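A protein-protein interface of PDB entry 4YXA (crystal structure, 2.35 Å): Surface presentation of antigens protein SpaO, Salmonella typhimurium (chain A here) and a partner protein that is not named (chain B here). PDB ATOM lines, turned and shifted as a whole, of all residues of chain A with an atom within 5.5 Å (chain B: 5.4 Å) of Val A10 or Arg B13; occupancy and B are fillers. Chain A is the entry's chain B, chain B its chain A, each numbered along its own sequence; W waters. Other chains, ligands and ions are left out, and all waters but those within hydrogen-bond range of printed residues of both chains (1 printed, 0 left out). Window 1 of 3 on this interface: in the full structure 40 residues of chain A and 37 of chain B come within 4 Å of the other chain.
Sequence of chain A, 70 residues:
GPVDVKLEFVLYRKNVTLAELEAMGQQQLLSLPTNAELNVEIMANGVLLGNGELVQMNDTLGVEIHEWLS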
ATOM      1  N   GLU A   8       0.463  -9.035  31.615  1.00  0.00           N
ATOM      2  CA  GLU A   8       1.114  -8.023  30.816  1.00  0.00           C
ATOM      3  C   GLU A   8       0.137  -6.914  30.552  1.00  0.00           C
ATOM      4  O   GLU A   8      -1.032  -7.155  30.286  1.00  0.00           O
ATOM      5  CB  GLU A   8       1.645  -8.597  29.505  1.00  0.00           C
ATOM      6  CG  GLU A   8       3.050  -9.174  29.600  1.00  0.00           C
ATOM      7  CD  GLU A   8       3.618  -9.533  28.235  1.00  0.00           C
ATOM      8  OE1 GLU A   8       2.811  -9.781  27.305  1.00  0.00           O
ATOM      9  OE2 GLU A   8       4.864  -9.565  28.091  1.00  0.00           O
ATOM     10  N   PHE A   9       0.646  -5.692  30.661  1.00  0.00           N
ATOM     11  CA  PHE A   9      -0.122  -4.486  30.434  1.00  0.00           C
ATOM     12  C   PHE A   9       0.290  -3.906  29.098  1.00  0.00           C
ATOM     13  O   PHE A   9       1.359  -3.343  28.939  1.00  0.00           O
ATOM     14  CB  PHE A   9       0.081  -3.504  31.579  1.00  0.00           C
ATOM     15  CG  PHE A   9      -0.488  -3.996  32.869  1.00  0.00           C
ATOM     16  CD1 PHE A   9      -1.830  -3.844  33.140  1.00  0.00           C
ATOM     17  CD2 PHE A   9       0.295  -4.666  33.777  1.00  0.00           C
ATOM     18  CE1 PHE A   9      -2.372  -4.315  34.314  1.00  0.00           C
ATOM     19  CE2 PHE A   9      -0.241  -5.137  34.950  1.00  0.00           C
ATOM     20  CZ  PHE A   9      -1.574  -4.959  35.218  1.00  0.00           C
ATOM     21  N   VAL A  10      -0.598  -4.087  28.140  1.00  0.00           N
ATOM     22  CA  VAL A  10      -0.347  -3.808  26.756  1.00  0.00           C
ATOM     23  C   VAL A  10      -1.038  -2.526  26.361  1.00  0.00           C
ATOM     24  O   VAL A  10      -2.267  -2.463  26.307  1.00  0.00           O
ATOM     25  CB  VAL A  10      -0.854  -4.962  25.881  1.00  0.00           C
ATOM     26  CG1 VAL A  10      -0.878  -4.559  24.431  1.00  0.00           C
ATOM     27  CG2 VAL A  10       0.003  -6.189  26.089  1.00  0.00           C
ATOM     28  N   LEU A  11      -0.253  -1.500  26.073  1.00  0.00           N
ATOM     29  CA  LEU A  11      -0.814  -0.215  25.696  1.00  0.00           C
ATOM     30  C   LEU A  11      -1.504  -0.272  24.341  1.00  0.00           C
ATOM     31  O   LEU A  11      -2.552   0.353  24.135  1.00  0.00           O
ATOM     32  CB  LEU A  11       0.275   0.852  25.676  1.00  0.00           C
ATOM     33  CG  LEU A  11      -0.209   2.283  25.438  1.00  0.00           C
ATOM     34  CD1 LEU A  11      -1.269   2.670  26.448  1.00  0.00           C
ATOM     35  CD2 LEU A  11       0.972   3.212  25.522  1.00  0.00           C
ATOM     36  N   TYR A  12      -0.918  -1.025  23.417  1.00  0.00           N
ATOM     37  CA  TYR A  12      -1.395  -1.030  22.048  1.00  0.00           C
ATOM     38  C   TYR A  12      -1.010  -2.324  21.348  1.00  0.00           C
ATOM     39  O   TYR A  12       0.051  -2.872  21.627  1.00  0.00           O
ATOM     40  CB  TYR A  12      -0.830   0.180  21.301  1.00  0.00           C
ATOM     41  CG  TYR A  12      -1.408   0.402  19.918  1.00  0.00           C
ATOM     42  CD1 TYR A  12      -2.723   0.806  19.751  1.00  0.00           C
ATOM     43  CD2 TYR A  12      -0.624   0.237  18.785  1.00  0.00           C
ATOM     44  CE1 TYR A  12      -3.246   1.012  18.506  1.00  0.00           C
ATOM     45  CE2 TYR A  12      -1.143   0.442  17.531  1.00  0.00           C
ATOM     46  CZ  TYR A  12      -2.453   0.829  17.397  1.00  0.00           C
ATOM     47  OH  TYR A  12      -2.968   1.033  16.142  1.00  0.00           O
ATOM     48  N   ARG A  13      -1.878  -2.817  20.462  1.00  0.00           N
ATOM     49  CA  ARG A  13      -1.556  -3.959  19.596  1.00  0.00           C
ATOM     50  C   ARG A  13      -1.824  -3.651  18.127  1.00  0.00           C
ATOM     51  O   ARG A  13      -2.763  -2.925  17.798  1.00  0.00           O
ATOM     52  CB  ARG A  13      -2.344  -5.196  20.002  1.00  0.00           C
ATOM     53  CG  ARG A  13      -1.956  -5.736  21.362  1.00  0.00           C
ATOM     54  CD  ARG A  13      -2.717  -7.007  21.691  1.00  0.00           C
ATOM     55  NE  ARG A  13      -4.155  -6.768  21.784  1.00  0.00           N
ATOM     56  CZ  ARG A  13      -5.077  -7.720  21.676  1.00  0.00           C
ATOM     57  NH1 ARG A  13      -4.711  -8.973  21.470  1.00  0.00           N
ATOM     58  NH2 ARG A  13      -6.361  -7.417  21.770  1.00  0.00           N
ATOM     59  N   LYS A  14      -1.001  -4.212  17.248  1.00  0.00           N
ATOM     60  CA  LYS A  14      -1.123  -3.956  15.815  1.00  0.00           C
ATOM     61  C   LYS A  14      -0.528  -5.094  14.977  1.00  0.00           C
ATOM     62  O   LYS A  14       0.610  -5.516  15.188  1.00  0.00           O
ATOM     63  CB  LYS A  14      -0.445  -2.620  15.452  1.00  0.00           C
ATOM     64  CG  LYS A  14      -0.482  -2.253  13.960  1.00  0.00           C
ATOM     65  CD  LYS A  14      -0.951  -0.821  13.738  1.00  0.00           C
ATOM     66  CE  LYS A  14      -1.807  -0.704  12.487  1.00  0.00           C
ATOM     67  NZ  LYS A  14      -2.276   0.693  12.237  1.00  0.00           N
ATOM     68  N   ASN A  39      -7.650   2.571  27.533  1.00  0.00           N
ATOM     69  CA  ASN A  39      -8.039   1.248  27.124  1.00  0.00           C
ATOM     70  C   ASN A  39      -6.817   0.377  27.099  1.00  0.00           C
ATOM     71  O   ASN A  39      -6.474  -0.206  26.076  1.00  0.00           O
ATOM     72  CB  ASN A  39      -8.720   1.276  25.762  1.00  0.00           C
ATOM     73  CG  ASN A  39      -9.497   0.014  25.486  1.00  0.00           C
ATOM     74  OD1 ASN A  39     -10.227  -0.478  26.350  1.00  0.00           O
ATOM     75  ND2 ASN A  39      -9.325  -0.541  24.288  1.00  0.00           N
ATOM     76  N   VAL A  40      -6.142   0.315  28.238  1.00  0.00           N
ATOM     77  CA  VAL A  40      -4.957  -0.518  28.387  1.00  0.00           C
ATOM     78  C   VAL A  40      -5.385  -1.977  28.471  1.00  0.00           C
ATOM     79  O   VAL A  40      -6.332  -2.320  29.175  1.00  0.00           O
ATOM     80  CB  VAL A  40      -4.152  -0.107  29.633  1.00  0.00           C
ATOM     81  CG1 VAL A  40      -3.003  -1.045  29.872  1.00  0.00           C
ATOM     82  CG2 VAL A  40      -3.646   1.281  29.454  1.00  0.00           C
ATOM     83  N   GLU A  41      -4.712  -2.837  27.733  1.00  0.00           N
ATOM     84  CA  GLU A  41      -5.102  -4.234  27.713  1.00  0.00           C
ATOM     85  C   GLU A  41      -4.279  -5.059  28.662  1.00  0.00           C
ATOM     86  O   GLU A  41      -3.093  -4.830  28.829  1.00  0.00           O
ATOM     87  CB  GLU A  41      -4.986  -4.798  26.304  1.00  0.00           C
ATOM     88  CG  GLU A  41      -6.045  -4.266  25.382  1.00  0.00           C
ATOM     89  CD  GLU A  41      -6.043  -4.983  24.084  1.00  0.00           C
ATOM     90  OE1 GLU A  41      -4.966  -5.495  23.731  1.00  0.00           O
ATOM     91  OE2 GLU A  41      -7.103  -5.045  23.423  1.00  0.00           O
ATOM     92  N   ILE A  42      -4.931  -6.031  29.278  1.00  0.00           N
ATOM     93  CA  ILE A  42      -4.268  -6.918  30.208  1.00  0.00           C
ATOM     94  C   ILE A  42      -4.279  -8.344  29.677  1.00  0.00           C
ATOM     95  O   ILE A  42      -5.324  -8.943  29.450  1.00  0.00           O
ATOM     96  CB  ILE A  42      -4.925  -6.861  31.578  1.00  0.00           C
ATOM     97  CG1 ILE A  42      -5.051  -5.409  32.006  1.00  0.00           C
ATOM     98  CG2 ILE A  42      -4.091  -7.606  32.578  1.00  0.00           C
ATOM     99  CD1 ILE A  42      -6.150  -5.191  32.996  1.00  0.00           C
ATOM    100  N   MET A  43      -3.089  -8.880  29.467  1.00  0.00           N
ATOM    101  CA  MET A  43      -2.967 -10.183  28.851  1.00  0.00           C
ATOM    102  C   MET A  43      -2.016 -11.055  29.622  1.00  0.00           C
ATOM    103  O   MET A  43      -1.039 -10.572  30.179  1.00  0.00           O
ATOM    104  CB  MET A  43      -2.496 -10.042  27.418  1.00  0.00           C
ATOM    105  CG  MET A  43      -3.387  -9.172  26.568  1.00  0.00           C
ATOM    106  SD  MET A  43      -2.449  -8.875  24.912  1.00  0.00           S
ATOM    107  CE  MET A  43      -1.639 -10.618  24.706  1.00  0.00           C
ATOM    108  N   GLY A  46      -0.629 -14.408  26.200  1.00  0.00           N
ATOM    109  CA  GLY A  46      -1.004 -14.079  24.844  1.00  0.00           C
ATOM    110  C   GLY A  46      -2.506 -14.213  24.773  1.00  0.00           C
ATOM    111  O   GLY A  46      -3.083 -14.456  23.716  1.00  0.00           O
ATOM    112  N   PRO B  11       1.622  -9.969  14.851  1.00  0.00           N
ATOM    113  CA  PRO B  11       1.012  -9.242  15.960  1.00  0.00           C
ATOM    114  C   PRO B  11       2.050  -8.720  16.951  1.00  0.00           C
ATOM    115  O   PRO B  11       2.717  -9.519  17.623  1.00  0.00           O
ATOM    116  CB  PRO B  11       0.111 -10.295  16.614  1.00  0.00           C
ATOM    117  CG  PRO B  11       0.689 -11.607  16.201  1.00  0.00           C
ATOM    118  CD  PRO B  11       1.220 -11.385  14.825  1.00  0.00           C
ATOM    119  N   LEU B  12       2.169  -7.390  17.033  1.00  0.00           N
ATOM    120  CA  LEU B  12       3.036  -6.710  18.011  1.00  0.00           C
ATOM    121  C   LEU B  12       2.254  -6.145  19.214  1.00  0.00           C
ATOM    122  O   LEU B  12       1.369  -5.304  19.036  1.00  0.00           O
ATOM    123  CB  LEU B  12       3.812  -5.561  17.346  1.00  0.00           C
ATOM    124  CG  LEU B  12       4.768  -5.878  16.189  1.00  0.00           C
ATOM    125  CD1 LEU B  12       5.416  -4.597  15.664  1.00  0.00           C
ATOM    126  CD2 LEU B  12       5.814  -6.924  16.563  1.00  0.00           C
ATOM    127  N   ARG B  13       2.579  -6.613  20.423  1.00  0.00           N
ATOM    128  CA  ARG B  13       2.083  -6.001  21.648  1.00  0.00           C
ATOM    129  C   ARG B  13       3.062  -4.955  22.096  1.00  0.00           C
ATOM    130  O   ARG B  13       4.240  -5.254  22.283  1.00  0.00           O
ATOM    131  CB  ARG B  13       1.918  -7.014  22.774  1.00  0.00           C
ATOM    132  CG  ARG B  13       1.200  -8.265  22.416  1.00  0.00           C
ATOM    133  CD  ARG B  13       1.413  -9.280  23.506  1.00  0.00           C
ATOM    134  NE  ARG B  13       2.716  -9.931  23.431  1.00  0.00           N
ATOM    135  CZ  ARG B  13       3.175 -10.768  24.357  1.00  0.00           C
ATOM    136  NH1 ARG B  13       2.442 -11.027  25.429  1.00  0.00           N
ATOM    137  NH2 ARG B  13       4.364 -11.339  24.227  1.00  0.00           N
ATOM    138  N   PHE B  14       2.587  -3.734  22.291  1.00  0.00           N
ATOM    139  CA  PHE B  14       3.423  -2.711  22.887  1.00  0.00           C
ATOM    140  C   PHE B  14       3.178  -2.671  24.389  1.00  0.00           C
ATOM    141  O   PHE B  14       2.204  -2.101  24.868  1.00  0.00           O
ATOM    142  CB  PHE B  14       3.162  -1.378  22.223  1.00  0.00           C
ATOM    143  CG  PHE B  14       3.653  -1.322  20.804  1.00  0.00           C
ATOM    144  CD1 PHE B  14       4.898  -0.787  20.507  1.00  0.00           C
ATOM    145  CD2 PHE B  14       2.889  -1.830  19.769  1.00  0.00           C
ATOM    146  CE1 PHE B  14       5.358  -0.740  19.205  1.00  0.00           C
ATOM    147  CE2 PHE B  14       3.349  -1.792  18.467  1.00  0.00           C
ATOM    148  CZ  PHE B  14       4.585  -1.244  18.188  1.00  0.00           C
ATOM    149  N   VAL B  15       4.079  -3.314  25.125  1.00  0.00           N
ATOM    150  CA  VAL B  15       3.881  -3.585  26.540  1.00  0.00           C
ATOM    151  C   VAL B  15       4.572  -2.550  27.410  1.00  0.00           C
ATOM    152  O   VAL B  15       5.709  -2.186  27.164  1.00  0.00           O
ATOM    153  CB  VAL B  15       4.392  -4.987  26.893  1.00  0.00           C
ATOM    154  CG1 VAL B  15       4.122  -5.299  28.351  1.00  0.00           C
ATOM    155  CG2 VAL B  15       3.721  -6.019  25.998  1.00  0.00           C
ATOM    156  N   ILE B  16       3.871  -2.085  28.433  1.00  0.00           N
ATOM    157  CA  ILE B  16       4.367  -1.013  29.282  1.00  0.00           C
ATOM    158  C   ILE B  16       4.665  -1.460  30.710  1.00  0.00           C
ATOM    159  O   ILE B  16       5.254  -0.724  31.487  1.00  0.00           O
ATOM    160  CB  ILE B  16       3.365   0.145  29.308  1.00  0.00           C
ATOM    161  CG1 ILE B  16       2.002  -0.356  29.792  1.00  0.00           C
ATOM    162  CG2 ILE B  16       3.268   0.764  27.917  1.00  0.00           C
ATOM    163  CD1 ILE B  16       0.985   0.731  29.981  1.00  0.00           C
ATOM    164  N   GLU B  43       8.145  -2.095  26.060  1.00  0.00           N
ATOM    165  CA  GLU B  43       8.694  -3.104  25.155  1.00  0.00           C
ATOM    166  C   GLU B  43       7.777  -3.722  24.112  1.00  0.00           C
ATOM    167  O   GLU B  43       6.581  -3.903  24.308  1.00  0.00           O
ATOM    168  CB  GLU B  43       9.289  -4.232  25.979  1.00  0.00           C
ATOM    169  CG  GLU B  43      10.689  -3.925  26.441  1.00  0.00           C
ATOM    170  CD  GLU B  43      11.430  -5.157  26.861  1.00  0.00           C
ATOM    171  OE1 GLU B  43      12.375  -5.550  26.130  1.00  0.00           O
ATOM    172  OE2 GLU B  43      11.054  -5.728  27.911  1.00  0.00           O
ATOM    173  N   VAL B  44       8.404  -4.077  23.002  1.00  0.00           N
ATOM    174  CA  VAL B  44       7.724  -4.598  21.838  1.00  0.00           C
ATOM    175  C   VAL B  44       7.936  -6.098  21.733  1.00  0.00           C
ATOM    176  O   VAL B  44       9.064  -6.569  21.612  1.00  0.00           O
ATOM    177  CB  VAL B  44       8.238  -3.916  20.565  1.00  0.00           C
ATOM    178  CG1 VAL B  44       7.341  -4.232  19.399  1.00  0.00           C
ATOM    179  CG2 VAL B  44       8.336  -2.417  20.782  1.00  0.00           C
ATOM    180  N   TYR B  45       6.850  -6.852  21.794  1.00  0.00           N
ATOM    181  CA  TYR B  45       6.936  -8.294  21.673  1.00  0.00           C
ATOM    182  C   TYR B  45       6.331  -8.736  20.379  1.00  0.00           C
ATOM    183  O   TYR B  45       5.333  -8.185  19.942  1.00  0.00           O
ATOM    184  CB  TYR B  45       6.189  -8.996  22.799  1.00  0.00           C
ATOM    185  CG  TYR B  45       6.883  -9.028  24.125  1.00  0.00           C
ATOM    186  CD1 TYR B  45       7.176 -10.225  24.736  1.00  0.00           C
ATOM    187  CD2 TYR B  45       7.252  -7.864  24.753  1.00  0.00           C
ATOM    188  CE1 TYR B  45       7.789 -10.261  25.943  1.00  0.00           C
ATOM    189  CE2 TYR B  45       7.872  -7.885  25.969  1.00  0.00           C
ATOM    190  CZ  TYR B  45       8.141  -9.086  26.561  1.00  0.00           C
ATOM    191  OH  TYR B  45       8.765  -9.109  27.785  1.00  0.00           O
ATOM    192  N   CYS B  46       6.915  -9.755  19.776  1.00  0.00           N
ATOM    193  CA  CYS B  46       6.149 -10.550  18.837  1.00  0.00           C
ATOM    194  C   CYS B  46       5.980 -11.908  19.479  1.00  0.00           C
ATOM    195  O   CYS B  46       6.955 -12.592  19.778  1.00  0.00           O
ATOM    196  CB  CYS B  46       6.820 -10.656  17.470  1.00  0.00           C
ATOM    197  SG  CYS B  46       5.693 -11.333  16.204  1.00  0.00           S
ATOM    198  N   TYR B  47       4.732 -12.282  19.697  1.00  0.00           N
ATOM    199  CA  TYR B  47       4.435 -13.431  20.524  1.00  0.00           C
ATOM    200  C   TYR B  47       5.287 -13.350  21.786  1.00  0.00           C
ATOM    201  O   TYR B  47       5.317 -12.310  22.438  1.00  0.00           O
ATOM    202  CB  TYR B  47       4.643 -14.725  19.735  1.00  0.00           C
ATOM    203  CG  TYR B  47       3.511 -14.929  18.749  1.00  0.00           C
ATOM    204  CD1 TYR B  47       2.338 -15.564  19.136  1.00  0.00           C
ATOM    205  CD2 TYR B  47       3.589 -14.435  17.451  1.00  0.00           C
ATOM    206  CE1 TYR B  47       1.288 -15.729  18.257  1.00  0.00           C
ATOM    207  CE2 TYR B  47       2.538 -14.601  16.559  1.00  0.00           C
ATOM    208  CZ  TYR B  47       1.385 -15.249  16.971  1.00  0.00           C
ATOM    209  OH  TYR B  47       0.320 -15.422  16.107  1.00  0.00           O
ATOM    210  N   ALA B  48       6.000 -14.407  22.130  1.00  0.00           N
ATOM    211  CA  ALA B  48       6.734 -14.372  23.384  1.00  0.00           C
ATOM    212  C   ALA B  48       8.171 -13.916  23.169  1.00  0.00           C
ATOM    213  O   ALA B  48       9.084 -14.314  23.889  1.00  0.00           O
ATOM    214  CB  ALA B  48       6.695 -15.736  24.055  1.00  0.00           C
ATOM    215  N   LYS B  49       8.377 -13.058  22.187  1.00  0.00           N
ATOM    216  CA  LYS B  49       9.732 -12.710  21.817  1.00  0.00           C
ATOM    217  C   LYS B  49       9.972 -11.212  21.882  1.00  0.00           C
ATOM    218  O   LYS B  49       9.269 -10.430  21.253  1.00  0.00           O
ATOM    219  CB  LYS B  49      10.021 -13.248  20.425  1.00  0.00           C
ATOM    220  CG  LYS B  49       9.735 -14.747  20.305  1.00  0.00           C
ATOM    221  CD  LYS B  49      10.691 -15.430  19.348  1.00  0.00           C
ATOM    222  CE  LYS B  49      11.098 -16.808  19.858  1.00  0.00           C
ATOM    223  NZ  LYS B  49      12.577 -17.047  19.771  1.00  0.00           N
HETATM  224  O   HOH W   1       0.555 -11.951  26.802  1.00  0.00           O
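O of Lys A14 sits at hydrogen-bond distance from N of Leu B12, 3.1 Å away. NH2 of Arg B13 lies within salt-bridge range of OE1 of Glu A8 (3.8 Å). The backbone carbonyl oxygen (O) of Phe B14 lies within hydrogen-bond range of the backbone NH (N) of Leu A11 (2.8 Å). The backbone NH (N) of Phe B14 is in hydrogen-bond range of the backbone carbonyl oxygen (O) of Tyr A12 (2.8 Å). N of Ile B16 lies within hydrogen-bond range of O of Phe A9.
O of Pro B11 lies within hydrogen-bond range of SG of Cys B46, 3.8 Å away. The backbone carbonyl oxygen (O) of Arg B13 is in hydrogen-bond range of the backbone NH (N) of Tyr B45, at 3.1 Å. The backbone NH (N) of Glu B43 sits at hydrogen-bond distance from the backbone carbonyl oxygen (O) of Val B15. The backbone NH of Glu A8 lies within hydrogen-bond range of the backbone carbonyl oxygen of Met A43 (2.6 Å). N of Val A10 lies within hydrogen-bond range of O of Glu A41, 2.7 Å away. The guanidinium group (NE) of Arg A13 lies within salt-bridge range of the side-chain carboxylate (OE1) of Glu A41 (2.5 Å).
Among the printed residues, pairs that only touch across the chains: Arg A13 with Leu B12, Phe A9 with Val B15, Met A43 with Arg B13, Val A10 with Phe B14, Glu A8 with Tyr B45, Tyr A12 with Arg B13, Val A10 with Val B15, Leu A11 with Ile B16, Tyr A12 with Leu B12, Lys A14 with Pro B11 and Val A10 with Arg B13.
Of the printed residues of chain B, Glu A8 touches Arg B13 (2.3 Å) and Tyr B45 (3.6 Å). Of the printed residues of chain B, Phe A9 touches Val B15 and Ile B16. Val A10 touches just these residues of chain B: Arg B13, Phe B14 and Val B15. Of the printed residues of chain B, Arg A13 touches Leu B12. Of chain A, only Glu A8 (2.3 Å), Val A10 (3.9 Å), Tyr A12 (3.7 Å) and Met A43 (3.5 Å) come within 4 Å of Arg B13. Of the printed residues of chain A, Tyr B45 touches Glu A8 (3.6 Å). The nearest residue of chain B that does not touch Val A10 is Ile B16 (4.8 Å).
Of the 13 printed residues of chain A, 8 touch a printed residue of chain B. Printed residues of chain A that touch a printed residue of chain B: Glu A8, Phe A9, Val A10, Leu A11, Tyr A12, Arg A13, Lys A14 and Met A43. Of the 13 printed residues of chain B, 7 touch a printed residue of chain A. Printed residues of chain B that touch a printed residue of chain A: Pro B11, Leu B12, Arg B13, Phe B14, Val B15, Ile B16 and Tyr B45. Among the printed residues, 16 pairs touch across the chains.
Water W1 lies within hydrogen-bond range of NH1 of Arg B13 (2.5 Å), N of Gly A46 (2.8 Å) and OE1 of Glu A8 (3.2 Å).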
